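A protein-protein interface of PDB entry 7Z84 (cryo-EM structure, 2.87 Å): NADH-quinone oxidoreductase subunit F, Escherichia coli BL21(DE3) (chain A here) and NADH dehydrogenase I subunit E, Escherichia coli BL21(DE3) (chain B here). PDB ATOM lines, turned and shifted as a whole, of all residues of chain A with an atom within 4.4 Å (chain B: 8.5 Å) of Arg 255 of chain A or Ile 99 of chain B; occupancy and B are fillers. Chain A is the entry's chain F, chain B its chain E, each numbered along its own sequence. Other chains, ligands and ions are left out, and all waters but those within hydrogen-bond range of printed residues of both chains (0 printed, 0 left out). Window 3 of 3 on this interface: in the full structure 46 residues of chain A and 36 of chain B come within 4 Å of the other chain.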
ATOM      1  N   GLY A 254      15.518 -25.603 -23.279  1.00  0.00           N
ATOM      2  CA  GLY A 254      14.225 -26.259 -23.245  1.00  0.00           C
ATOM      3  C   GLY A 254      13.290 -25.795 -22.146  1.00  0.00           C
ATOM      4  O   GLY A 254      13.385 -26.260 -21.006  1.00  0.00           O
ATOM      5  N   ARG A 255      12.363 -24.899 -22.510  1.00  0.00           N
ATOM      6  CA  ARG A 255      11.298 -24.390 -21.632  1.00  0.00           C
ATOM      7  C   ARG A 255      11.834 -23.835 -20.315  1.00  0.00           C
ATOM      8  O   ARG A 255      11.245 -24.028 -19.250  1.00  0.00           O
ATOM      9  CB  ARG A 255      10.229 -25.453 -21.379  1.00  0.00           C
ATOM     10  CG  ARG A 255       9.860 -26.255 -22.605  1.00  0.00           C
ATOM     11  CD  ARG A 255       8.716 -27.203 -22.323  1.00  0.00           C
ATOM     12  NE  ARG A 255       7.555 -26.909 -23.151  1.00  0.00           N
ATOM     13  CZ  ARG A 255       6.356 -27.446 -22.974  1.00  0.00           C
ATOM     14  NH1 ARG A 255       6.127 -28.319 -22.007  1.00  0.00           N
ATOM     15  NH2 ARG A 255       5.364 -27.098 -23.788  1.00  0.00           N
ATOM     16  N   VAL A 256      12.959 -23.136 -20.387  1.00  0.00           N
ATOM     17  CA  VAL A 256      13.486 -22.400 -19.252  1.00  0.00           C
ATOM     18  C   VAL A 256      13.280 -20.912 -19.519  1.00  0.00           C
ATOM     19  O   VAL A 256      12.917 -20.500 -20.621  1.00  0.00           O
ATOM     20  CB  VAL A 256      14.964 -22.732 -18.976  1.00  0.00           C
ATOM     21  CG1 VAL A 256      15.087 -24.144 -18.435  1.00  0.00           C
ATOM     22  CG2 VAL A 256      15.780 -22.586 -20.236  1.00  0.00           C
ATOM     23  N   MET A 281      12.951 -23.111 -14.457  1.00  0.00           N
ATOM     24  CA  MET A 281      11.904 -23.564 -15.357  1.00  0.00           C
ATOM     25  C   MET A 281      10.882 -22.449 -15.583  1.00  0.00           C
ATOM     26  O   MET A 281      10.815 -21.466 -14.840  1.00  0.00           O
ATOM     27  CB  MET A 281      11.222 -24.809 -14.793  1.00  0.00           C
ATOM     28  CG  MET A 281      12.097 -26.056 -14.795  1.00  0.00           C
ATOM     29  SD  MET A 281      12.813 -26.469 -16.396  1.00  0.00           S
ATOM     30  CE  MET A 281      11.338 -26.713 -17.374  1.00  0.00           C
ATOM     31  N   ARG A 282      10.076 -22.611 -16.629  1.00  0.00           N
ATOM     32  CA  ARG A 282       9.070 -21.616 -16.963  1.00  0.00           C
ATOM     33  C   ARG A 282       7.892 -21.700 -15.992  1.00  0.00           C
ATOM     34  O   ARG A 282       7.824 -22.571 -15.121  1.00  0.00           O
ATOM     35  CB  ARG A 282       8.605 -21.789 -18.407  1.00  0.00           C
ATOM     36  CG  ARG A 282       9.551 -21.195 -19.433  1.00  0.00           C
ATOM     37  CD  ARG A 282       8.788 -20.516 -20.557  1.00  0.00           C
ATOM     38  NE  ARG A 282       8.004 -21.465 -21.337  1.00  0.00           N
ATOM     39  CZ  ARG A 282       8.377 -21.958 -22.510  1.00  0.00           C
ATOM     40  NH1 ARG A 282       9.524 -21.614 -23.071  1.00  0.00           N
ATOM     41  NH2 ARG A 282       7.577 -22.816 -23.136  1.00  0.00           N
ATOM     42  N   LEU A 285       5.511 -25.015 -15.047  1.00  0.00           N
ATOM     43  CA  LEU A 285       6.253 -26.223 -15.367  1.00  0.00           C
ATOM     44  C   LEU A 285       7.187 -26.571 -14.217  1.00  0.00           C
ATOM     45  O   LEU A 285       7.849 -25.692 -13.656  1.00  0.00           O
ATOM     46  CB  LEU A 285       7.060 -26.055 -16.658  1.00  0.00           C
ATOM     47  CG  LEU A 285       6.297 -25.540 -17.879  1.00  0.00           C
ATOM     48  CD1 LEU A 285       7.226 -25.404 -19.071  1.00  0.00           C
ATOM     49  CD2 LEU A 285       5.132 -26.453 -18.209  1.00  0.00           C
ATOM     50  N   MET A 327      20.039 -30.058 -21.374  1.00  0.00           N
ATOM     51  CA  MET A 327      18.687 -29.898 -21.887  1.00  0.00           C
ATOM     52  C   MET A 327      17.711 -30.386 -20.829  1.00  0.00           C
ATOM     53  O   MET A 327      17.818 -31.522 -20.359  1.00  0.00           O
ATOM     54  CB  MET A 327      18.511 -30.658 -23.205  1.00  0.00           C
ATOM     55  CG  MET A 327      17.151 -30.510 -23.847  1.00  0.00           C
ATOM     56  SD  MET A 327      16.638 -32.039 -24.646  1.00  0.00           S
ATOM     57  CE  MET A 327      16.554 -33.150 -23.248  1.00  0.00           C
ATOM     58  N   ALA A 328      16.772 -29.523 -20.454  1.00  0.00           N
ATOM     59  CA  ALA A 328      15.863 -29.774 -19.344  1.00  0.00           C
ATOM     60  C   ALA A 328      14.509 -30.251 -19.847  1.00  0.00           C
ATOM     61  O   ALA A 328      13.947 -29.686 -20.790  1.00  0.00           O
ATOM     62  CB  ALA A 328      15.684 -28.515 -18.493  1.00  0.00           C
ATOM     63  N   VAL A 329      13.988 -31.294 -19.205  1.00  0.00           N
ATOM     64  CA  VAL A 329      12.691 -31.877 -19.519  1.00  0.00           C
ATOM     65  C   VAL A 329      11.766 -31.618 -18.342  1.00  0.00           C
ATOM     66  O   VAL A 329      12.102 -31.956 -17.199  1.00  0.00           O
ATOM     67  CB  VAL A 329      12.807 -33.386 -19.792  1.00  0.00           C
ATOM     68  CG1 VAL A 329      11.590 -33.882 -20.540  1.00  0.00           C
ATOM     69  CG2 VAL A 329      14.082 -33.697 -20.547  1.00  0.00           C
ATOM     70  N   ASP A 330      10.602 -31.038 -18.621  1.00  0.00           N
ATOM     71  CA  ASP A 330       9.619 -30.717 -17.599  1.00  0.00           C
ATOM     72  C   ASP A 330       8.648 -31.883 -17.421  1.00  0.00           C
ATOM     73  O   ASP A 330       8.813 -32.957 -18.006  1.00  0.00           O
ATOM     74  CB  ASP A 330       8.881 -29.428 -17.955  1.00  0.00           C
ATOM     75  CG  ASP A 330       8.473 -29.376 -19.411  1.00  0.00           C
ATOM     76  OD1 ASP A 330       9.199 -29.939 -20.255  1.00  0.00           O
ATOM     77  OD2 ASP A 330       7.421 -28.775 -19.711  1.00  0.00           O
ATOM     78  N   GLU A 332       5.479 -31.961 -18.336  1.00  0.00           N
ATOM     79  CA  GLU A 332       4.504 -32.095 -19.413  1.00  0.00           C
ATOM     80  C   GLU A 332       4.973 -33.028 -20.520  1.00  0.00           C
ATOM     81  O   GLU A 332       4.151 -33.463 -21.333  1.00  0.00           O
ATOM     82  CB  GLU A 332       4.177 -30.726 -20.010  1.00  0.00           C
ATOM     83  CG  GLU A 332       3.546 -29.750 -19.036  1.00  0.00           C
ATOM     84  CD  GLU A 332       2.394 -28.983 -19.654  1.00  0.00           C
ATOM     85  OE1 GLU A 332       1.565 -29.610 -20.346  1.00  0.00           O
ATOM     86  OE2 GLU A 332       2.318 -27.754 -19.452  1.00  0.00           O
ATOM     87  N   ILE A 333       6.262 -33.345 -20.575  1.00  0.00           N
ATOM     88  CA  ILE A 333       6.805 -34.150 -21.662  1.00  0.00           C
ATOM     89  C   ILE A 333       6.788 -35.618 -21.256  1.00  0.00           C
ATOM     90  O   ILE A 333       7.340 -35.993 -20.217  1.00  0.00           O
ATOM     91  CB  ILE A 333       8.225 -33.694 -22.029  1.00  0.00           C
ATOM     92  CG1 ILE A 333       8.223 -32.217 -22.439  1.00  0.00           C
ATOM     93  CG2 ILE A 333       8.821 -34.596 -23.105  1.00  0.00           C
ATOM     94  CD1 ILE A 333       7.880 -31.968 -23.894  1.00  0.00           C
ATOM     95  N   LEU A 338       9.795 -38.642 -25.837  1.00  0.00           N
ATOM     96  CA  LEU A 338      11.116 -38.026 -25.910  1.00  0.00           C
ATOM     97  C   LEU A 338      12.175 -39.034 -26.339  1.00  0.00           C
ATOM     98  O   LEU A 338      13.008 -38.748 -27.211  1.00  0.00           O
ATOM     99  CB  LEU A 338      11.474 -37.424 -24.553  1.00  0.00           C
ATOM    100  CG  LEU A 338      12.562 -36.360 -24.559  1.00  0.00           C
ATOM    101  CD1 LEU A 338      11.999 -35.083 -25.131  1.00  0.00           C
ATOM    102  CD2 LEU A 338      13.083 -36.136 -23.162  1.00  0.00           C
ATOM    103  N   ASP B  93      13.263 -31.558 -36.134  1.00  0.00           N
ATOM    104  CA  ASP B  93      12.441 -32.497 -35.380  1.00  0.00           C
ATOM    105  C   ASP B  93      13.244 -33.199 -34.291  1.00  0.00           C
ATOM    106  O   ASP B  93      12.894 -34.304 -33.871  1.00  0.00           O
ATOM    107  CB  ASP B  93      11.772 -33.517 -36.308  1.00  0.00           C
ATOM    108  CG  ASP B  93      12.759 -34.417 -37.034  1.00  0.00           C
ATOM    109  OD1 ASP B  93      13.977 -34.158 -37.012  1.00  0.00           O
ATOM    110  OD2 ASP B  93      12.303 -35.405 -37.644  1.00  0.00           O
ATOM    111  N   SER B  94      14.319 -32.574 -33.824  1.00  0.00           N
ATOM    112  CA  SER B  94      15.179 -33.194 -32.829  1.00  0.00           C
ATOM    113  C   SER B  94      14.607 -32.957 -31.432  1.00  0.00           C
ATOM    114  O   SER B  94      13.491 -32.460 -31.270  1.00  0.00           O
ATOM    115  CB  SER B  94      16.608 -32.682 -32.972  1.00  0.00           C
ATOM    116  OG  SER B  94      17.219 -33.198 -34.141  1.00  0.00           O
ATOM    117  N   VAL B  95      15.383 -33.309 -30.404  1.00  0.00           N
ATOM    118  CA  VAL B  95      14.827 -33.499 -29.066  1.00  0.00           C
ATOM    119  C   VAL B  95      14.461 -32.165 -28.413  1.00  0.00           C
ATOM    120  O   VAL B  95      13.416 -32.052 -27.759  1.00  0.00           O
ATOM    121  CB  VAL B  95      15.800 -34.338 -28.212  1.00  0.00           C
ATOM    122  CG1 VAL B  95      17.195 -33.718 -28.152  1.00  0.00           C
ATOM    123  CG2 VAL B  95      15.242 -34.588 -26.825  1.00  0.00           C
ATOM    124  N   VAL B  96      15.289 -31.132 -28.590  1.00  0.00           N
ATOM    125  CA  VAL B  96      15.009 -29.847 -27.953  1.00  0.00           C
ATOM    126  C   VAL B  96      13.818 -29.166 -28.614  1.00  0.00           C
ATOM    127  O   VAL B  96      12.981 -28.559 -27.938  1.00  0.00           O
ATOM    128  CB  VAL B  96      16.259 -28.950 -27.972  1.00  0.00           C
ATOM    129  CG1 VAL B  96      16.098 -27.798 -26.996  1.00  0.00           C
ATOM    130  CG2 VAL B  96      17.488 -29.764 -27.636  1.00  0.00           C
ATOM    131  N   CYS B  97      13.719 -29.253 -29.941  1.00  0.00           N
ATOM    132  CA  CYS B  97      12.562 -28.695 -30.626  1.00  0.00           C
ATOM    133  C   CYS B  97      11.316 -29.546 -30.429  1.00  0.00           C
ATOM    134  O   CYS B  97      10.202 -29.030 -30.561  1.00  0.00           O
ATOM    135  CB  CYS B  97      12.867 -28.522 -32.112  1.00  0.00           C
ATOM    136  SG  CYS B  97      14.153 -27.297 -32.442  1.00  0.00           S
ATOM    137  N   HIS B  98      11.480 -30.836 -30.126  1.00  0.00           N
ATOM    138  CA  HIS B  98      10.349 -31.638 -29.669  1.00  0.00           C
ATOM    139  C   HIS B  98       9.868 -31.167 -28.305  1.00  0.00           C
ATOM    140  O   HIS B  98       8.662 -31.152 -28.035  1.00  0.00           O
ATOM    141  CB  HIS B  98      10.737 -33.116 -29.627  1.00  0.00           C
ATOM    142  CG  HIS B  98       9.729 -33.990 -28.950  1.00  0.00           C
ATOM    143  ND1 HIS B  98       8.653 -34.538 -29.614  1.00  0.00           N
ATOM    144  CD2 HIS B  98       9.635 -34.417 -27.669  1.00  0.00           C
ATOM    145  CE1 HIS B  98       7.939 -35.262 -28.771  1.00  0.00           C
ATOM    146  NE2 HIS B  98       8.513 -35.204 -27.584  1.00  0.00           N
ATOM    147  N   ILE B  99      10.805 -30.799 -27.427  1.00  0.00           N
ATOM    148  CA  ILE B  99      10.449 -30.216 -26.137  1.00  0.00           C
ATOM    149  C   ILE B  99       9.752 -28.874 -26.336  1.00  0.00           C
ATOM    150  O   ILE B  99       8.739 -28.581 -25.688  1.00  0.00           O
ATOM    151  CB  ILE B  99      11.705 -30.096 -25.253  1.00  0.00           C
ATOM    152  CG1 ILE B  99      12.058 -31.455 -24.650  1.00  0.00           C
ATOM    153  CG2 ILE B  99      11.525 -29.070 -24.157  1.00  0.00           C
ATOM    154  CD1 ILE B  99      13.185 -31.414 -23.645  1.00  0.00           C
ATOM    155  N   ASN B 100      10.252 -28.062 -27.264  1.00  0.00           N
ATOM    156  CA  ASN B 100       9.649 -26.770 -27.563  1.00  0.00           C
ATOM    157  C   ASN B 100       8.431 -26.875 -28.471  1.00  0.00           C
ATOM    158  O   ASN B 100       7.844 -25.843 -28.813  1.00  0.00           O
ATOM    159  CB  ASN B 100      10.685 -25.841 -28.198  1.00  0.00           C
ATOM    160  CG  ASN B 100      11.803 -25.481 -27.244  1.00  0.00           C
ATOM    161  OD1 ASN B 100      12.981 -25.618 -27.570  1.00  0.00           O
ATOM    162  ND2 ASN B 100      11.441 -25.017 -26.055  1.00  0.00           N
ATOM    163  N   GLY B 101       8.037 -28.083 -28.868  1.00  0.00           N
ATOM    164  CA  GLY B 101       6.818 -28.273 -29.626  1.00  0.00           C
ATOM    165  C   GLY B 101       6.926 -27.989 -31.109  1.00  0.00           C
ATOM    166  O   GLY B 101       6.284 -27.065 -31.614  1.00  0.00           O
ATOM    167  N   TYR B 102       7.735 -28.776 -31.821  1.00  0.00           N
ATOM    168  CA  TYR B 102       7.782 -28.663 -33.273  1.00  0.00           C
ATOM    169  C   TYR B 102       6.547 -29.247 -33.943  1.00  0.00           C
ATOM    170  O   TYR B 102       6.336 -28.990 -35.132  1.00  0.00           O
ATOM    171  CB  TYR B 102       9.039 -29.350 -33.829  1.00  0.00           C
ATOM    172  CG  TYR B 102       8.905 -30.848 -34.055  1.00  0.00           C
ATOM    173  CD1 TYR B 102       9.122 -31.745 -33.021  1.00  0.00           C
ATOM    174  CD2 TYR B 102       8.594 -31.364 -35.312  1.00  0.00           C
ATOM    175  CE1 TYR B 102       9.006 -33.107 -33.220  1.00  0.00           C
ATOM    176  CE2 TYR B 102       8.462 -32.719 -35.516  1.00  0.00           C
ATOM    177  CZ  TYR B 102       8.681 -33.587 -34.468  1.00  0.00           C
ATOM    178  OH  TYR B 102       8.566 -34.943 -34.671  1.00  0.00           O
ATOM    179  N   GLN B 103       5.754 -30.049 -33.225  1.00  0.00           N
ATOM    180  CA  GLN B 103       4.627 -30.736 -33.848  1.00  0.00           C
ATOM    181  C   GLN B 103       3.524 -29.771 -34.253  1.00  0.00           C
ATOM    182  O   GLN B 103       2.854 -29.997 -35.265  1.00  0.00           O
ATOM    183  CB  GLN B 103       4.078 -31.808 -32.910  1.00  0.00           C
ATOM    184  CG  GLN B 103       4.929 -33.060 -32.851  1.00  0.00           C
ATOM    185  CD  GLN B 103       5.730 -33.158 -31.571  1.00  0.00           C
ATOM    186  OE1 GLN B 103       6.162 -32.149 -31.014  1.00  0.00           O
ATOM    187  NE2 GLN B 103       5.931 -34.379 -31.095  1.00  0.00           N
ATOM    188  N   CYS B 137      19.131 -24.563 -30.696  1.00  0.00           N
ATOM    189  CA  CYS B 137      18.219 -25.181 -29.739  1.00  0.00           C
ATOM    190  C   CYS B 137      17.748 -24.198 -28.677  1.00  0.00           C
ATOM    191  O   CYS B 137      16.655 -24.362 -28.126  1.00  0.00           O
ATOM    192  CB  CYS B 137      18.895 -26.383 -29.089  1.00  0.00           C
ATOM    193  SG  CYS B 137      19.932 -27.306 -30.230  1.00  0.00           S
ATOM    194  N   ASP B 138      18.551 -23.177 -28.373  1.00  0.00           N
ATOM    195  CA  ASP B 138      18.143 -22.173 -27.400  1.00  0.00           C
ATOM    196  C   ASP B 138      17.063 -21.242 -27.934  1.00  0.00           C
ATOM    197  O   ASP B 138      16.426 -20.542 -27.140  1.00  0.00           O
ATOM    198  CB  ASP B 138      19.356 -21.356 -26.952  1.00  0.00           C
ATOM    199  CG  ASP B 138      20.267 -20.983 -28.104  1.00  0.00           C
ATOM    200  OD1 ASP B 138      19.951 -21.349 -29.255  1.00  0.00           O
ATOM    201  OD2 ASP B 138      21.299 -20.326 -27.858  1.00  0.00           O
ATOM    202  N   GLY B 140      14.603 -22.481 -30.160  1.00  0.00           N
ATOM    203  CA  GLY B 140      13.715 -23.404 -30.825  1.00  0.00           C
ATOM    204  C   GLY B 140      12.250 -23.056 -30.645  1.00  0.00           C
ATOM    205  O   GLY B 140      11.884 -22.277 -29.760  1.00  0.00           O
ATOM    206  N   PRO B 141      11.373 -23.626 -31.490  1.00  0.00           N
ATOM    207  CA  PRO B 141      11.665 -24.513 -32.624  1.00  0.00           C
ATOM    208  C   PRO B 141      12.198 -23.765 -33.846  1.00  0.00           C
ATOM    209  O   PRO B 141      11.963 -22.566 -33.976  1.00  0.00           O
ATOM    210  CB  PRO B 141      10.307 -25.149 -32.930  1.00  0.00           C
ATOM    211  CG  PRO B 141       9.319 -24.161 -32.452  1.00  0.00           C
ATOM    212  CD  PRO B 141       9.926 -23.493 -31.257  1.00  0.00           C
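Of chain B, only Ile 99 (3.3 Å) and Asn 100 (3.7 Å) come within 4 Å of Arg 255 of chain A. No residue of chain B comes within 4 Å of Val 256 of chain A. Of the printed residues of chain B, Met 327 of chain A touches Val 95, Val 96 and Ile 99. Printed residues of chain B within 4 Å of Ala 328 of chain A: Ile 99. Of the printed residues of chain B, Leu 338 of chain A touches Val 95, His 98 and Ile 99. Of the printed residues of chain A, Val 95 of chain B touches Met 327 (3.6 Å) and Leu 338 (3.7 Å). Of the printed residues of chain A, Ile 99 of chain B touches Arg 255 (3.3 Å), Met 327 (3.6 Å), Ala 328 (3.4 Å), Val 329 (3.95 Å), Ile 333 (3.8 Å) and Leu 338 (3.7 Å). Of the printed residues of chain A, Asn 100 of chain B touches Arg 255. Pro 141 of chain B touches none of the printed residues of chain A.
The backbone carbonyl oxygen (O) of Ile 99 of chain B lies within hydrogen-bond range of the guanidinium group (NE) of Arg 255 of chain A.
Of the 13 printed residues of chain A, 6 touch a printed residue of chain B. Printed residues of chain A that touch a printed residue of chain B: Arg 255, Met 327, Ala 328, Val 329, Ile 333 and Leu 338. Along chain A the printed residues that touch a printed residue of chain B span positions 255 to 338. Of the 15 printed residues of chain B, 5 touch a printed residue of chain A. Among the printed residues, no Asp or Glu carboxylate lies within 4 Å of a Lys or Arg side-chain nitrogen of the other chain.
ND2 of Asn 100 of chain B touches N of Arg 255 of chain A, 3.7 Å away. CG2 of Val 95 of chain B touches SD of Met 327 of chain A, 3.6 Å away. SD of Met 327 of chain A touches CG2 of Val 96 of chain B, at 3.9 Å. Met 327 of chain A touches Ile 99 of chain B (SD to CD1, 3.6 Å). Ala 328 of chain A touches Ile 99 of chain B (O to CD1, 3.4 Å). Val 329 of chain A touches Ile 99 of chain B (CG2 to CD1, 3.95 Å). Ile 333 of chain A touches Ile 99 of chain B (CD1 to CA, 3.8 Å). Val 95 of chain B touches Leu 338 of chain A (CG2 to CD1, 3.7 Å). Leu 338 of chain A touches His 98 of chain B (CD1 to CD2, 3.5 Å). CD1 of Leu 338 of chain A touches CG1 of Ile 99 of chain B (3.7 Å).
A ring nitrogen (ND1) of His 98 of chain B is in hydrogen-bond range of the side-chain amide nitrogen (NE2) of Gln 103 of chain B, 3.1 Å away. The backbone carbonyl oxygen (O) of Arg 255 of chain A sits at hydrogen-bond distance from the backbone NH (N) of Arg 282 of chain A (3.2 Å). The side-chain carboxylate (OD2) of Asp 330 of chain A lies within salt-bridge range of the guanidinium group (NH1) of Arg 255 of chain A, at 2.7 Å. O of Val 96 of chain B sits close to OD1 of Asn 100 of chain B, 3.0 Å away.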
